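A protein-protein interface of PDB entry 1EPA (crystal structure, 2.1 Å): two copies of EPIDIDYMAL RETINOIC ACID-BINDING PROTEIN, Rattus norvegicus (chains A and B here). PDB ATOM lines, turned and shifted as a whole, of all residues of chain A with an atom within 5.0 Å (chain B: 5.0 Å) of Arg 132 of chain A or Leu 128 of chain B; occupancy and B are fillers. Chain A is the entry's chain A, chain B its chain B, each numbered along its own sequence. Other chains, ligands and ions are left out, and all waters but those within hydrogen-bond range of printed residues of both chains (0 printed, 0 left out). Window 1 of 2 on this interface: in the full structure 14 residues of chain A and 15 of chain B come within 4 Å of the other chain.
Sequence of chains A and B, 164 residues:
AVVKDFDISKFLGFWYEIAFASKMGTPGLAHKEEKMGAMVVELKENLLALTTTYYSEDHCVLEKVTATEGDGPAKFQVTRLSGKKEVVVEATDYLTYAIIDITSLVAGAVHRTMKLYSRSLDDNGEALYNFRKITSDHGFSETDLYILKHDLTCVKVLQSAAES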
ATOM      1  N   LEU A 128      -2.692  23.891  -5.425  1.00  0.00           N
ATOM      2  CA  LEU A 128      -3.010  22.560  -4.928  1.00  0.00           C
ATOM      3  C   LEU A 128      -2.155  21.486  -5.538  1.00  0.00           C
ATOM      4  O   LEU A 128      -1.780  20.506  -4.888  1.00  0.00           O
ATOM      5  CB  LEU A 128      -4.456  22.188  -5.170  1.00  0.00           C
ATOM      6  CG  LEU A 128      -5.368  22.698  -4.078  1.00  0.00           C
ATOM      7  CD1 LEU A 128      -6.726  22.990  -4.660  1.00  0.00           C
ATOM      8  CD2 LEU A 128      -5.299  21.699  -2.911  1.00  0.00           C
ATOM      9  N   TYR A 129      -1.756  21.700  -6.765  1.00  0.00           N
ATOM     10  CA  TYR A 129      -0.879  20.749  -7.424  1.00  0.00           C
ATOM     11  C   TYR A 129       0.473  20.913  -6.810  1.00  0.00           C
ATOM     12  O   TYR A 129       1.127  19.915  -6.587  1.00  0.00           O
ATOM     13  CB  TYR A 129      -0.823  21.044  -8.908  1.00  0.00           C
ATOM     14  CG  TYR A 129       0.092  20.112  -9.686  1.00  0.00           C
ATOM     15  CD1 TYR A 129       0.084  18.751  -9.446  1.00  0.00           C
ATOM     16  CD2 TYR A 129       0.929  20.684 -10.620  1.00  0.00           C
ATOM     17  CE1 TYR A 129       0.932  17.951 -10.152  1.00  0.00           C
ATOM     18  CE2 TYR A 129       1.779  19.866 -11.324  1.00  0.00           C
ATOM     19  CZ  TYR A 129       1.767  18.512 -11.083  1.00  0.00           C
ATOM     20  OH  TYR A 129       2.614  17.703 -11.821  1.00  0.00           O
ATOM     21  N   ASN A 130       0.949  22.101  -6.518  1.00  0.00           N
ATOM     22  CA  ASN A 130       2.198  22.219  -5.781  1.00  0.00           C
ATOM     23  C   ASN A 130       2.097  21.596  -4.387  1.00  0.00           C
ATOM     24  O   ASN A 130       2.995  20.959  -3.850  1.00  0.00           O
ATOM     25  CB  ASN A 130       2.577  23.663  -5.663  1.00  0.00           C
ATOM     26  CG  ASN A 130       3.525  23.978  -6.796  1.00  0.00           C
ATOM     27  OD1 ASN A 130       4.570  23.329  -6.932  1.00  0.00           O
ATOM     28  ND2 ASN A 130       3.263  24.947  -7.676  1.00  0.00           N
ATOM     29  N   PHE A 131       0.934  21.654  -3.785  1.00  0.00           N
ATOM     30  CA  PHE A 131       0.704  21.064  -2.492  1.00  0.00           C
ATOM     31  C   PHE A 131       0.855  19.602  -2.619  1.00  0.00           C
ATOM     32  O   PHE A 131       1.512  19.035  -1.733  1.00  0.00           O
ATOM     33  CB  PHE A 131      -0.690  21.331  -1.948  1.00  0.00           C
ATOM     34  CG  PHE A 131      -0.794  21.021  -0.480  1.00  0.00           C
ATOM     35  CD1 PHE A 131       0.054  21.607   0.413  1.00  0.00           C
ATOM     36  CD2 PHE A 131      -1.795  20.186  -0.047  1.00  0.00           C
ATOM     37  CE1 PHE A 131      -0.120  21.360   1.741  1.00  0.00           C
ATOM     38  CE2 PHE A 131      -1.950  19.956   1.275  1.00  0.00           C
ATOM     39  CZ  PHE A 131      -1.116  20.547   2.160  1.00  0.00           C
ATOM     40  N   ARG A 132       0.341  19.007  -3.696  1.00  0.00           N
ATOM     41  CA  ARG A 132       0.510  17.573  -3.820  1.00  0.00           C
ATOM     42  C   ARG A 132       1.956  17.155  -3.983  1.00  0.00           C
ATOM     43  O   ARG A 132       2.361  16.168  -3.370  1.00  0.00           O
ATOM     44  CB  ARG A 132      -0.325  17.014  -4.994  1.00  0.00           C
ATOM     45  CG  ARG A 132      -1.753  17.212  -4.631  1.00  0.00           C
ATOM     46  CD  ARG A 132      -2.670  16.839  -5.724  1.00  0.00           C
ATOM     47  NE  ARG A 132      -4.055  16.994  -5.304  1.00  0.00           N
ATOM     48  CZ  ARG A 132      -4.722  15.981  -4.774  1.00  0.00           C
ATOM     49  NH1 ARG A 132      -4.162  14.793  -4.592  1.00  0.00           N
ATOM     50  NH2 ARG A 132      -5.998  16.130  -4.467  1.00  0.00           N
ATOM     51  N   LYS A 133       2.747  17.884  -4.757  1.00  0.00           N
ATOM     52  CA  LYS A 133       4.174  17.608  -4.932  1.00  0.00           C
ATOM     53  C   LYS A 133       4.961  17.819  -3.652  1.00  0.00           C
ATOM     54  O   LYS A 133       5.746  16.946  -3.257  1.00  0.00           O
ATOM     55  CB  LYS A 133       4.772  18.495  -6.033  1.00  0.00           C
ATOM     56  CG  LYS A 133       4.374  18.017  -7.437  1.00  0.00           C
ATOM     57  CD  LYS A 133       4.874  19.009  -8.482  1.00  0.00           C
ATOM     58  CE  LYS A 133       6.350  19.419  -8.326  1.00  0.00           C
ATOM     59  NZ  LYS A 133       6.778  20.261  -9.440  1.00  0.00           N
ATOM     60  N   ILE A 134       4.717  18.896  -2.907  1.00  0.00           N
ATOM     61  CA  ILE A 134       5.453  19.086  -1.672  1.00  0.00           C
ATOM     62  C   ILE A 134       4.947  18.120  -0.644  1.00  0.00           C
ATOM     63  O   ILE A 134       5.833  17.620   0.040  1.00  0.00           O
ATOM     64  CB  ILE A 134       5.328  20.601  -1.245  1.00  0.00           C
ATOM     65  CG1 ILE A 134       6.384  21.331  -2.044  1.00  0.00           C
ATOM     66  CG2 ILE A 134       5.550  20.889   0.230  1.00  0.00           C
ATOM     67  CD1 ILE A 134       6.212  22.865  -2.092  1.00  0.00           C
ATOM     68  N   THR A 135       3.687  17.714  -0.439  1.00  0.00           N
ATOM     69  CA  THR A 135       3.459  16.738   0.600  1.00  0.00           C
ATOM     70  C   THR A 135       3.975  15.364   0.181  1.00  0.00           C
ATOM     71  O   THR A 135       4.467  14.661   1.071  1.00  0.00           O
ATOM     72  CB  THR A 135       1.957  16.666   0.992  1.00  0.00           C
ATOM     73  OG1 THR A 135       1.226  16.388  -0.160  1.00  0.00           O
ATOM     74  CG2 THR A 135       1.430  17.936   1.581  1.00  0.00           C
ATOM     75  N   SER A 136       3.953  14.866  -1.061  1.00  0.00           N
ATOM     76  CA  SER A 136       4.526  13.550  -1.351  1.00  0.00           C
ATOM     77  C   SER A 136       6.005  13.571  -1.019  1.00  0.00           C
ATOM     78  O   SER A 136       6.421  12.640  -0.339  1.00  0.00           O
ATOM     79  CB  SER A 136       4.406  13.163  -2.796  1.00  0.00           C
ATOM     80  OG  SER A 136       4.710  14.351  -3.491  1.00  0.00           O
ATOM     81  N   GLU A 142      -1.302  10.400  -1.054  1.00  0.00           N
ATOM     82  CA  GLU A 142      -2.509  11.046  -1.575  1.00  0.00           C
ATOM     83  C   GLU A 142      -3.709  10.809  -0.671  1.00  0.00           C
ATOM     84  O   GLU A 142      -4.602  11.641  -0.574  1.00  0.00           O
ATOM     85  CB  GLU A 142      -2.865  10.512  -2.951  1.00  0.00           C
ATOM     86  CG  GLU A 142      -4.033  11.266  -3.555  1.00  0.00           C
ATOM     87  CD  GLU A 142      -4.250  10.904  -5.015  1.00  0.00           C
ATOM     88  OE1 GLU A 142      -3.310  11.102  -5.779  1.00  0.00           O
ATOM     89  OE2 GLU A 142      -5.332  10.424  -5.368  1.00  0.00           O
ATOM     90  N   LEU A 145      -4.099  13.502   2.112  1.00  0.00           N
ATOM     91  CA  LEU A 145      -4.499  14.865   1.809  1.00  0.00           C
ATOM     92  C   LEU A 145      -6.010  15.051   1.942  1.00  0.00           C
ATOM     93  O   LEU A 145      -6.775  14.166   1.515  1.00  0.00           O
ATOM     94  CB  LEU A 145      -4.146  15.268   0.380  1.00  0.00           C
ATOM     95  CG  LEU A 145      -2.731  15.120  -0.161  1.00  0.00           C
ATOM     96  CD1 LEU A 145      -2.509  16.177  -1.265  1.00  0.00           C
ATOM     97  CD2 LEU A 145      -1.726  15.245   0.985  1.00  0.00           C
ATOM     98  N   ILE A 147      -9.008  17.959   1.205  1.00  0.00           N
ATOM     99  CA  ILE A 147      -9.318  19.216   0.551  1.00  0.00           C
ATOM    100  C   ILE A 147     -10.629  19.623   1.223  1.00  0.00           C
ATOM    101  O   ILE A 147     -11.585  18.832   1.308  1.00  0.00           O
ATOM    102  CB  ILE A 147      -9.448  18.938  -0.953  1.00  0.00           C
ATOM    103  CG1 ILE A 147      -8.117  18.366  -1.469  1.00  0.00           C
ATOM    104  CG2 ILE A 147      -9.775  20.246  -1.711  1.00  0.00           C
ATOM    105  CD1 ILE A 147      -8.289  17.517  -2.732  1.00  0.00           C
ATOM    106  N   ILE B  18     -12.157   9.273  -8.756  1.00  0.00           N
ATOM    107  CA  ILE B  18     -11.346  10.210  -8.011  1.00  0.00           C
ATOM    108  C   ILE B  18     -12.017  11.558  -7.774  1.00  0.00           C
ATOM    109  O   ILE B  18     -11.830  12.153  -6.715  1.00  0.00           O
ATOM    110  CB  ILE B  18     -10.017  10.370  -8.810  1.00  0.00           C
ATOM    111  CG1 ILE B  18      -9.310   9.029  -8.833  1.00  0.00           C
ATOM    112  CG2 ILE B  18      -9.071  11.396  -8.189  1.00  0.00           C
ATOM    113  CD1 ILE B  18      -8.908   8.402  -7.511  1.00  0.00           C
ATOM    114  N   ALA B  19     -12.750  12.104  -8.730  1.00  0.00           N
ATOM    115  CA  ALA B  19     -13.352  13.412  -8.592  1.00  0.00           C
ATOM    116  C   ALA B  19     -14.508  13.518  -9.555  1.00  0.00           C
ATOM    117  O   ALA B  19     -14.600  12.749 -10.536  1.00  0.00           O
ATOM    118  CB  ALA B  19     -12.372  14.514  -8.949  1.00  0.00           C
ATOM    119  N   LEU B 116     -13.481  12.219 -13.095  1.00  0.00           N
ATOM    120  CA  LEU B 116     -12.108  11.795 -13.339  1.00  0.00           C
ATOM    121  C   LEU B 116     -11.984  10.369 -12.852  1.00  0.00           C
ATOM    122  O   LEU B 116     -12.197  10.116 -11.681  1.00  0.00           O
ATOM    123  CB  LEU B 116     -11.061  12.696 -12.589  1.00  0.00           C
ATOM    124  CG  LEU B 116      -9.623  12.222 -12.310  1.00  0.00           C
ATOM    125  CD1 LEU B 116      -8.915  11.796 -13.565  1.00  0.00           C
ATOM    126  CD2 LEU B 116      -8.864  13.366 -11.729  1.00  0.00           C
ATOM    127  N   ASN B 124      -2.127  10.933  -8.521  1.00  0.00           N
ATOM    128  CA  ASN B 124      -3.169  11.509  -9.359  1.00  0.00           C
ATOM    129  C   ASN B 124      -3.011  13.015  -9.470  1.00  0.00           C
ATOM    130  O   ASN B 124      -3.938  13.667  -9.940  1.00  0.00           O
ATOM    131  CB  ASN B 124      -4.548  11.257  -8.815  1.00  0.00           C
ATOM    132  CG  ASN B 124      -4.938   9.814  -8.949  1.00  0.00           C
ATOM    133  OD1 ASN B 124      -4.840   9.214 -10.005  1.00  0.00           O
ATOM    134  ND2 ASN B 124      -5.434   9.164  -7.920  1.00  0.00           N
ATOM    135  N   GLY B 125      -1.842  13.592  -9.138  1.00  0.00           N
ATOM    136  CA  GLY B 125      -1.638  15.040  -9.070  1.00  0.00           C
ATOM    137  C   GLY B 125      -1.898  15.755 -10.401  1.00  0.00           C
ATOM    138  O   GLY B 125      -2.594  16.773 -10.524  1.00  0.00           O
ATOM    139  N   GLU B 126      -1.342  15.065 -11.400  1.00  0.00           N
ATOM    140  CA  GLU B 126      -1.297  15.540 -12.769  1.00  0.00           C
ATOM    141  C   GLU B 126      -2.698  15.362 -13.318  1.00  0.00           C
ATOM    142  O   GLU B 126      -3.314  16.339 -13.750  1.00  0.00           O
ATOM    143  CB  GLU B 126      -0.188  14.751 -13.495  1.00  0.00           C
ATOM    144  CG  GLU B 126       1.253  14.896 -12.828  1.00  0.00           C
ATOM    145  CD  GLU B 126       1.525  14.401 -11.351  1.00  0.00           C
ATOM    146  OE1 GLU B 126       0.982  13.354 -10.924  1.00  0.00           O
ATOM    147  OE2 GLU B 126       2.290  15.070 -10.608  1.00  0.00           O
ATOM    148  N   ALA B 127      -3.311  14.218 -13.162  1.00  0.00           N
ATOM    149  CA  ALA B 127      -4.693  14.054 -13.560  1.00  0.00           C
ATOM    150  C   ALA B 127      -5.632  15.106 -12.951  1.00  0.00           C
ATOM    151  O   ALA B 127      -6.430  15.711 -13.701  1.00  0.00           O
ATOM    152  CB  ALA B 127      -5.206  12.667 -13.150  1.00  0.00           C
ATOM    153  N   LEU B 128      -5.500  15.422 -11.657  1.00  0.00           N
ATOM    154  CA  LEU B 128      -6.451  16.327 -11.002  1.00  0.00           C
ATOM    155  C   LEU B 128      -6.246  17.759 -11.424  1.00  0.00           C
ATOM    156  O   LEU B 128      -7.225  18.476 -11.561  1.00  0.00           O
ATOM    157  CB  LEU B 128      -6.346  16.203  -9.473  1.00  0.00           C
ATOM    158  CG  LEU B 128      -6.969  14.908  -8.880  1.00  0.00           C
ATOM    159  CD1 LEU B 128      -6.331  14.547  -7.541  1.00  0.00           C
ATOM    160  CD2 LEU B 128      -8.465  15.124  -8.603  1.00  0.00           C
ATOM    161  N   TYR B 129      -5.023  18.207 -11.665  1.00  0.00           N
ATOM    162  CA  TYR B 129      -4.745  19.544 -12.189  1.00  0.00           C
ATOM    163  C   TYR B 129      -5.407  19.732 -13.582  1.00  0.00           C
ATOM    164  O   TYR B 129      -6.050  20.752 -13.904  1.00  0.00           O
ATOM    165  CB  TYR B 129      -3.184  19.648 -12.181  1.00  0.00           C
ATOM    166  CG  TYR B 129      -2.683  21.009 -12.680  1.00  0.00           C
ATOM    167  CD1 TYR B 129      -2.931  22.129 -11.906  1.00  0.00           C
ATOM    168  CD2 TYR B 129      -2.018  21.104 -13.892  1.00  0.00           C
ATOM    169  CE1 TYR B 129      -2.527  23.369 -12.318  1.00  0.00           C
ATOM    170  CE2 TYR B 129      -1.609  22.359 -14.308  1.00  0.00           C
ATOM    171  CZ  TYR B 129      -1.867  23.468 -13.517  1.00  0.00           C
ATOM    172  OH  TYR B 129      -1.419  24.706 -13.915  1.00  0.00           O
ATOM    173  N   ASN B 130      -5.281  18.678 -14.415  1.00  0.00           N
ATOM    174  CA  ASN B 130      -5.921  18.581 -15.729  1.00  0.00           C
ATOM    175  C   ASN B 130      -7.414  18.682 -15.674  1.00  0.00           C
ATOM    176  O   ASN B 130      -8.012  19.402 -16.490  1.00  0.00           O
ATOM    177  CB  ASN B 130      -5.648  17.277 -16.450  1.00  0.00           C
ATOM    178  CG  ASN B 130      -4.296  17.329 -17.104  1.00  0.00           C
ATOM    179  OD1 ASN B 130      -3.535  18.282 -16.951  1.00  0.00           O
ATOM    180  ND2 ASN B 130      -3.837  16.330 -17.823  1.00  0.00           N
ATOM    181  N   PHE B 131      -7.996  17.939 -14.726  1.00  0.00           N
ATOM    182  CA  PHE B 131      -9.421  17.940 -14.501  1.00  0.00           C
ATOM    183  C   PHE B 131      -9.871  19.288 -13.960  1.00  0.00           C
ATOM    184  O   PHE B 131     -10.906  19.774 -14.408  1.00  0.00           O
ATOM    185  CB  PHE B 131      -9.809  16.871 -13.511  1.00  0.00           C
ATOM    186  CG  PHE B 131     -11.300  16.716 -13.299  1.00  0.00           C
ATOM    187  CD1 PHE B 131     -12.068  16.121 -14.246  1.00  0.00           C
ATOM    188  CD2 PHE B 131     -11.871  17.078 -12.125  1.00  0.00           C
ATOM    189  CE1 PHE B 131     -13.392  15.874 -14.006  1.00  0.00           C
ATOM    190  CE2 PHE B 131     -13.207  16.833 -11.897  1.00  0.00           C
ATOM    191  CZ  PHE B 131     -13.969  16.224 -12.831  1.00  0.00           C
ATOM    192  N   ARG B 132      -9.169  19.933 -13.023  1.00  0.00           N
ATOM    193  CA  ARG B 132      -9.514  21.284 -12.626  1.00  0.00           C
ATOM    194  C   ARG B 132      -9.413  22.191 -13.868  1.00  0.00           C
ATOM    195  O   ARG B 132     -10.323  23.006 -14.017  1.00  0.00           O
ATOM    196  CB  ARG B 132      -8.554  21.759 -11.522  1.00  0.00           C
ATOM    197  CG  ARG B 132      -8.996  21.291 -10.135  1.00  0.00           C
ATOM    198  CD  ARG B 132      -8.087  21.726  -8.928  1.00  0.00           C
ATOM    199  NE  ARG B 132      -8.749  21.498  -7.645  1.00  0.00           N
ATOM    200  CZ  ARG B 132      -8.406  20.535  -6.784  1.00  0.00           C
ATOM    201  NH1 ARG B 132      -7.389  19.628  -6.956  1.00  0.00           N
ATOM    202  NH2 ARG B 132      -9.165  20.486  -5.698  1.00  0.00           N
ATOM    203  N   ILE B 147     -13.819  16.176  -4.573  1.00  0.00           N
ATOM    204  CA  ILE B 147     -12.700  15.246  -4.599  1.00  0.00           C
ATOM    205  C   ILE B 147     -13.086  14.170  -3.610  1.00  0.00           C
ATOM    206  O   ILE B 147     -13.335  14.466  -2.460  1.00  0.00           O
ATOM    207  CB  ILE B 147     -11.453  15.976  -4.170  1.00  0.00           C
ATOM    208  CG1 ILE B 147     -11.308  17.362  -4.885  1.00  0.00           C
ATOM    209  CG2 ILE B 147     -10.298  15.051  -4.472  1.00  0.00           C
ATOM    210  CD1 ILE B 147     -11.015  17.470  -6.404  1.00  0.00           C
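Among the printed residues, pairs that only touch across the chains: Arg 132 of chain A with Leu 128 of chain B, Tyr 129 of chain A with Gly 125 of chain B, Ile 147 of chain A with Ile 147 of chain B, Leu 128 of chain A with Arg 132 of chain B, Tyr 129 of chain A with Tyr 129 of chain B and Arg 132 of chain A with Gly 125 of chain B.
O of Arg 132 of chain A sits at hydrogen-bond distance from OG1 of Thr 135 of chain A, at 3.4 Å. O of Arg 132 of chain A lies within hydrogen-bond range of OG of Ser 136 of chain A (3.0 Å). NH1 of Arg 132 of chain A lies within salt-bridge range of OE1 of Glu 142 of chain A, 3.97 Å away.
Leu 128 of chain A touches Arg 132 of chain B, and with the chains exchanged Arg 132 of chain A touches Leu 128 of chain B. Tyr 129 of chain B touches its own counterpart, Tyr 129 of chain A. Ile 147 of chain A touches its own counterpart, Ile 147 of chain B. Positions printed for both chains: 128, 129, 130, 131, 132 and 147.
Of the 13 printed residues of chain B, 7 touch a printed residue of chain A. Printed residues of chain B that touch a printed residue of chain A: Asn 124, Gly 125, Glu 126, Leu 128, Tyr 129, Arg 132 and Ile 147. Hydrophobic or aromatic side chains of chain B within 4 Å of the printed part of chain A: Leu 128, Tyr 129 and Ile 147. Of the 12 printed residues of chain A, 5 touch a printed residue of chain B. Among the printed residues, no Asp or Glu carboxylate lies within 4 Å of a Lys or Arg side-chain nitrogen of the other chain.
Arg 132 of chain A touches just these residues of chain B: Gly 125 (3.9 Å) and Leu 128 (3.5 Å). Of chain A, only Arg 132 comes within 4 Å of Leu 128 of chain B. Of the printed residues of chain A, Asn 124 of chain B touches Glu 142. Printed residues of chain B within 4 Å of Glu 142 of chain A: Asn 124 (2.8 Å). Of the printed residues of chain B, Leu 128 of chain A touches Arg 132 (3.6 Å). The nearest residue of chain A that does not touch Leu 128 of chain B is Glu 142 of chain A (4.8 Å).
The side-chain hydroxyl (OH) of Tyr 129 of chain A lies within hydrogen-bond range of the side-chain carboxylate (OE2) of Glu 126 of chain B. OE2 of Glu 142 of chain A lies within hydrogen-bond range of ND2 of Asn 124 of chain B.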
